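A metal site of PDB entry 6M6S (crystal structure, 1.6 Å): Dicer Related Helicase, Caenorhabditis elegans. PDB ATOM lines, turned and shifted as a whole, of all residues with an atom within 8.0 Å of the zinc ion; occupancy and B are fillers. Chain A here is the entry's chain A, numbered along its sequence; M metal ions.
The side-chain sulfur (SG) of Cys 17 sits close to the backbone NH (N) of Lys 19 (3.7 Å). The backbone carbonyl oxygen (O) of Leu 74 lies within hydrogen-bond range of the backbone NH (N) of Cys 69, 2.9 Å away. The side-chain sulfur (SG) of Cys 69 sits close to the backbone NH (N) of His 71, at 3.5 Å. N of Asn 16 sits close to SG of Cys 14 (3.5 Å). The backbone NH of Leu 74 sits close to the side-chain sulfur of Cys 72 (3.7 Å). The backbone carbonyl oxygen (O) of Lys 19 sits at hydrogen-bond distance from the backbone NH (N) of Cys 14 (2.8 Å). SG of Cys 72 lies close to ND2 of Asn 16, 3.3 Å away.
Of the 20 residues printed, 4 come within 4 Å of the zinc ion.
The side-chain sulfur (SG) of Cys 17 is bound to the zinc ion. SG of Cys 69 is bound to the zinc ion (2.3 Å). The side-chain sulfur (SG) of Cys 72 binds the zinc ion. SG of Cys 14 is bound to the zinc ion (2.4 Å).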
ATOM      1  N   MET A  13     -15.372 -18.075  -2.827  1.00  0.00           N
ATOM      2  CA  MET A  13     -14.181 -18.943  -2.826  1.00  0.00           C
ATOM      3  C   MET A  13     -13.257 -18.560  -3.934  1.00  0.00           C
ATOM      4  O   MET A  13     -13.665 -17.989  -4.967  1.00  0.00           O
ATOM      5  CB  MET A  13     -14.598 -20.371  -3.133  1.00  0.00           C
ATOM      6  CG  MET A  13     -15.961 -20.474  -2.678  1.00  0.00           C
ATOM      7  SD  MET A  13     -15.767 -21.280  -1.136  1.00  0.00           S
ATOM      8  CE  MET A  13     -16.187 -22.606  -2.337  1.00  0.00           C
ATOM      9  N   CYS A  14     -11.972 -18.917  -3.773  1.00  0.00           N
ATOM     10  CA  CYS A  14     -11.016 -18.735  -4.875  1.00  0.00           C
ATOM     11  C   CYS A  14     -11.447 -19.600  -6.026  1.00  0.00           C
ATOM     12  O   CYS A  14     -11.631 -20.801  -5.845  1.00  0.00           O
ATOM     13  CB  CYS A  14      -9.621 -19.229  -4.370  1.00  0.00           C
ATOM     14  SG  CYS A  14      -8.329 -19.056  -5.659  1.00  0.00           S
ATOM     15  N   SER A  15     -11.519 -18.999  -7.216  1.00  0.00           N
ATOM     16  CA  SER A  15     -11.932 -19.749  -8.428  1.00  0.00           C
ATOM     17  C   SER A  15     -10.947 -20.840  -8.833  1.00  0.00           C
ATOM     18  O   SER A  15     -11.299 -21.791  -9.472  1.00  0.00           O
ATOM     19  CB  SER A  15     -12.140 -18.761  -9.606  1.00  0.00           C
ATOM     20  OG  SER A  15     -10.954 -17.992  -9.903  1.00  0.00           O
ATOM     21  N   ASN A  16      -9.707 -20.706  -8.406  1.00  0.00           N
ATOM     22  CA  ASN A  16      -8.662 -21.655  -8.758  1.00  0.00           C
ATOM     23  C   ASN A  16      -8.548 -22.804  -7.765  1.00  0.00           C
ATOM     24  O   ASN A  16      -8.579 -23.951  -8.178  1.00  0.00           O
ATOM     25  CB  ASN A  16      -7.300 -20.936  -8.794  1.00  0.00           C
ATOM     26  CG  ASN A  16      -6.177 -21.862  -9.228  1.00  0.00           C
ATOM     27  OD1 ASN A  16      -6.309 -22.603 -10.216  1.00  0.00           O
ATOM     28  ND2 ASN A  16      -5.092 -21.869  -8.510  1.00  0.00           N
ATOM     29  N   CYS A  17      -8.369 -22.506  -6.464  1.00  0.00           N
ATOM     30  CA  CYS A  17      -8.117 -23.582  -5.485  1.00  0.00           C
ATOM     31  C   CYS A  17      -9.301 -23.957  -4.548  1.00  0.00           C
ATOM     32  O   CYS A  17      -9.170 -24.884  -3.760  1.00  0.00           O
ATOM     33  CB  CYS A  17      -6.908 -23.261  -4.600  1.00  0.00           C
ATOM     34  SG  CYS A  17      -7.219 -21.888  -3.415  1.00  0.00           S
ATOM     35  N   SER A  18     -10.379 -23.194  -4.655  1.00  0.00           N
ATOM     36  CA  SER A  18     -11.623 -23.384  -3.906  1.00  0.00           C
ATOM     37  C   SER A  18     -11.546 -23.153  -2.405  1.00  0.00           C
ATOM     38  O   SER A  18     -12.418 -23.637  -1.686  1.00  0.00           O
ATOM     39  CB  SER A  18     -12.231 -24.771  -4.135  1.00  0.00           C
ATOM     40  OG  SER A  18     -12.509 -24.899  -5.522  1.00  0.00           O
ATOM     41  N   LYS A  19     -10.526 -22.450  -1.927  1.00  0.00           N
ATOM     42  CA  LYS A  19     -10.537 -22.065  -0.524  1.00  0.00           C
ATOM     43  C   LYS A  19     -11.465 -20.869  -0.328  1.00  0.00           C
ATOM     44  O   LYS A  19     -11.618 -20.005  -1.192  1.00  0.00           O
ATOM     45  CB  LYS A  19      -9.122 -21.647  -0.093  1.00  0.00           C
ATOM     46  CG  LYS A  19      -8.126 -22.808   0.037  1.00  0.00           C
ATOM     47  CD  LYS A  19      -8.451 -23.729   1.197  1.00  0.00           C
ATOM     48  CE  LYS A  19      -7.310 -24.722   1.365  1.00  0.00           C
ATOM     49  NZ  LYS A  19      -7.538 -25.650   2.498  1.00  0.00           N
ATOM     50  N   GLU A  20     -12.025 -20.811   0.880  1.00  0.00           N
ATOM     51  CA  GLU A  20     -13.068 -19.824   1.186  1.00  0.00           C
ATOM     52  C   GLU A  20     -12.432 -18.502   1.595  1.00  0.00           C
ATOM     53  O   GLU A  20     -11.477 -18.527   2.409  1.00  0.00           O
ATOM     54  CB  GLU A  20     -13.900 -20.415   2.334  1.00  0.00           C
ATOM     55  CG  GLU A  20     -15.000 -19.484   2.812  1.00  0.00           C
ATOM     56  CD  GLU A  20     -15.770 -19.999   4.050  1.00  0.00           C
ATOM     57  OE1 GLU A  20     -15.563 -21.138   4.515  1.00  0.00           O
ATOM     58  OE2 GLU A  20     -16.625 -19.190   4.541  1.00  0.00           O
ATOM     59  N   PHE A  21     -12.910 -17.374   1.073  1.00  0.00           N
ATOM     60  CA  PHE A  21     -12.433 -16.056   1.576  1.00  0.00           C
ATOM     61  C   PHE A  21     -13.437 -15.470   2.563  1.00  0.00           C
ATOM     62  O   PHE A  21     -13.024 -15.038   3.647  1.00  0.00           O
ATOM     63  CB  PHE A  21     -12.340 -15.105   0.419  1.00  0.00           C
ATOM     64  CG  PHE A  21     -11.252 -15.446  -0.547  1.00  0.00           C
ATOM     65  CD1 PHE A  21      -9.948 -15.700  -0.123  1.00  0.00           C
ATOM     66  CD2 PHE A  21     -11.471 -15.435  -1.935  1.00  0.00           C
ATOM     67  CE1 PHE A  21      -8.899 -15.996  -1.040  1.00  0.00           C
ATOM     68  CE2 PHE A  21     -10.441 -15.768  -2.844  1.00  0.00           C
ATOM     69  CZ  PHE A  21      -9.141 -16.006  -2.395  1.00  0.00           C
ATOM     70  N   PHE A  44      -6.797 -14.823   4.898  1.00  0.00           N
ATOM     71  CA  PHE A  44      -6.734 -15.644   3.698  1.00  0.00           C
ATOM     72  C   PHE A  44      -6.129 -14.932   2.497  1.00  0.00           C
ATOM     73  O   PHE A  44      -6.249 -15.379   1.360  1.00  0.00           O
ATOM     74  CB  PHE A  44      -8.201 -16.121   3.398  1.00  0.00           C
ATOM     75  CG  PHE A  44      -8.789 -16.753   4.639  1.00  0.00           C
ATOM     76  CD1 PHE A  44      -8.180 -17.882   5.204  1.00  0.00           C
ATOM     77  CD2 PHE A  44      -9.904 -16.169   5.273  1.00  0.00           C
ATOM     78  CE1 PHE A  44      -8.620 -18.419   6.451  1.00  0.00           C
ATOM     79  CE2 PHE A  44     -10.358 -16.706   6.518  1.00  0.00           C
ATOM     80  CZ  PHE A  44      -9.721 -17.833   7.086  1.00  0.00           C
ATOM     81  N   LYS A  68      -3.186 -11.588  -2.905  1.00  0.00           N
ATOM     82  CA  LYS A  68      -3.078 -12.914  -3.521  1.00  0.00           C
ATOM     83  C   LYS A  68      -3.773 -13.913  -2.631  1.00  0.00           C
ATOM     84  O   LYS A  68      -3.805 -13.805  -1.402  1.00  0.00           O
ATOM     85  CB  LYS A  68      -1.612 -13.330  -3.658  1.00  0.00           C
ATOM     86  CG  LYS A  68      -0.622 -12.177  -4.103  1.00  0.00           C
ATOM     87  CD  LYS A  68      -0.940 -11.707  -5.549  1.00  0.00           C
ATOM     88  CE  LYS A  68       0.142 -10.648  -5.912  1.00  0.00           C
ATOM     89  NZ  LYS A  68      -0.008 -10.209  -7.363  1.00  0.00           N
ATOM     90  N   CYS A  69      -4.319 -14.953  -3.247  1.00  0.00           N
ATOM     91  CA  CYS A  69      -4.891 -16.047  -2.429  1.00  0.00           C
ATOM     92  C   CYS A  69      -3.782 -16.625  -1.529  1.00  0.00           C
ATOM     93  O   CYS A  69      -2.687 -17.028  -2.004  1.00  0.00           O
ATOM     94  CB  CYS A  69      -5.470 -17.094  -3.386  1.00  0.00           C
ATOM     95  SG  CYS A  69      -6.029 -18.643  -2.511  1.00  0.00           S
ATOM     96  N   PHE A  70      -4.129 -16.754  -0.232  1.00  0.00           N
ATOM     97  CA  PHE A  70      -3.165 -17.309   0.733  1.00  0.00           C
ATOM     98  C   PHE A  70      -2.680 -18.701   0.374  1.00  0.00           C
ATOM     99  O   PHE A  70      -1.540 -19.057   0.684  1.00  0.00           O
ATOM    100  CB  PHE A  70      -3.742 -17.347   2.171  1.00  0.00           C
ATOM    101  CG  PHE A  70      -4.738 -18.464   2.388  1.00  0.00           C
ATOM    102  CD1 PHE A  70      -6.005 -18.412   1.789  1.00  0.00           C
ATOM    103  CD2 PHE A  70      -4.396 -19.600   3.117  1.00  0.00           C
ATOM    104  CE1 PHE A  70      -6.919 -19.427   1.963  1.00  0.00           C
ATOM    105  CE2 PHE A  70      -5.327 -20.611   3.306  1.00  0.00           C
ATOM    106  CZ  PHE A  70      -6.572 -20.524   2.738  1.00  0.00           C
ATOM    107  N   HIS A  71      -3.529 -19.518  -0.267  1.00  0.00           N
ATOM    108  CA  HIS A  71      -3.179 -20.882  -0.518  1.00  0.00           C
ATOM    109  C   HIS A  71      -2.521 -21.102  -1.903  1.00  0.00           C
ATOM    110  O   HIS A  71      -1.458 -21.759  -1.942  1.00  0.00           O
ATOM    111  CB  HIS A  71      -4.476 -21.698  -0.404  1.00  0.00           C
ATOM    112  CG  HIS A  71      -4.267 -23.165  -0.602  1.00  0.00           C
ATOM    113  ND1 HIS A  71      -3.619 -23.957   0.314  1.00  0.00           N
ATOM    114  CD2 HIS A  71      -4.623 -23.971  -1.639  1.00  0.00           C
ATOM    115  CE1 HIS A  71      -3.579 -25.205  -0.139  1.00  0.00           C
ATOM    116  NE2 HIS A  71      -4.190 -25.238  -1.308  1.00  0.00           N
ATOM    117  N   CYS A  72      -3.141 -20.577  -2.982  1.00  0.00           N
ATOM    118  CA  CYS A  72      -2.619 -20.898  -4.340  1.00  0.00           C
ATOM    119  C   CYS A  72      -1.766 -19.721  -4.925  1.00  0.00           C
ATOM    120  O   CYS A  72      -1.135 -19.868  -5.996  1.00  0.00           O
ATOM    121  CB  CYS A  72      -3.763 -21.272  -5.315  1.00  0.00           C
ATOM    122  SG  CYS A  72      -4.779 -19.938  -5.860  1.00  0.00           S
ATOM    123  N   LYS A  73      -1.802 -18.584  -4.228  1.00  0.00           N
ATOM    124  CA  LYS A  73      -1.034 -17.394  -4.574  1.00  0.00           C
ATOM    125  C   LYS A  73      -1.429 -16.663  -5.851  1.00  0.00           C
ATOM    126  O   LYS A  73      -0.712 -15.756  -6.287  1.00  0.00           O
ATOM    127  CB  LYS A  73       0.487 -17.683  -4.595  1.00  0.00           C
ATOM    128  CG  LYS A  73       0.971 -18.300  -3.248  1.00  0.00           C
ATOM    129  CD  LYS A  73       2.492 -18.453  -3.312  1.00  0.00           C
ATOM    130  CE  LYS A  73       3.052 -19.162  -2.062  1.00  0.00           C
ATOM    131  NZ  LYS A  73       4.560 -19.226  -2.081  1.00  0.00           N
ATOM    132  N   LEU A  74      -2.524 -17.039  -6.492  1.00  0.00           N
ATOM    133  CA  LEU A  74      -2.975 -16.244  -7.643  1.00  0.00           C
ATOM    134  C   LEU A  74      -3.412 -14.871  -7.182  1.00  0.00           C
ATOM    135  O   LEU A  74      -3.948 -14.666  -6.061  1.00  0.00           O
ATOM    136  CB  LEU A  74      -4.191 -16.943  -8.228  1.00  0.00           C
ATOM    137  CG  LEU A  74      -3.760 -17.805  -9.421  1.00  0.00           C
ATOM    138  CD1 LEU A  74      -2.649 -18.860  -9.123  1.00  0.00           C
ATOM    139  CD2 LEU A  74      -5.016 -18.453  -9.941  1.00  0.00           C
ATOM    140  N   ASP A  75      -3.232 -13.881  -8.060  1.00  0.00           N
ATOM    141  CA  ASP A  75      -3.787 -12.577  -7.711  1.00  0.00           C
ATOM    142  C   ASP A  75      -5.308 -12.546  -7.733  1.00  0.00           C
ATOM    143  O   ASP A  75      -5.959 -13.018  -8.704  1.00  0.00           O
ATOM    144  CB  ASP A  75      -3.297 -11.583  -8.741  1.00  0.00           C
ATOM    145  CG  ASP A  75      -3.635 -10.164  -8.317  1.00  0.00           C
ATOM    146  OD1 ASP A  75      -4.772  -9.718  -8.464  1.00  0.00           O
ATOM    147  OD2 ASP A  75      -2.726  -9.461  -7.804  1.00  0.00           O
ATOM    148  N   VAL A  76      -5.897 -12.001  -6.660  1.00  0.00           N
ATOM    149  CA  VAL A  76      -7.365 -11.999  -6.497  1.00  0.00           C
ATOM    150  C   VAL A  76      -7.966 -10.583  -6.342  1.00  0.00           C
ATOM    151  O   VAL A  76      -9.171 -10.452  -6.078  1.00  0.00           O
ATOM    152  CB  VAL A  76      -7.832 -12.921  -5.344  1.00  0.00           C
ATOM    153  CG1 VAL A  76      -7.424 -14.387  -5.662  1.00  0.00           C
ATOM    154  CG2 VAL A  76      -7.274 -12.412  -3.960  1.00  0.00           C
ATOM    155  N   ALA A  94     -12.069 -13.515 -10.011  1.00  0.00           N
ATOM    156  CA  ALA A  94     -11.295 -14.469  -9.208  1.00  0.00           C
ATOM    157  C   ALA A  94     -12.157 -15.350  -8.320  1.00  0.00           C
ATOM    158  O   ALA A  94     -11.575 -16.135  -7.529  1.00  0.00           O
ATOM    159  CB  ALA A  94     -10.318 -13.679  -8.275  1.00  0.00           C
HETATM  160 ZN    ZN M   1      -6.555 -19.926  -4.338  1.00  0.00          ZN
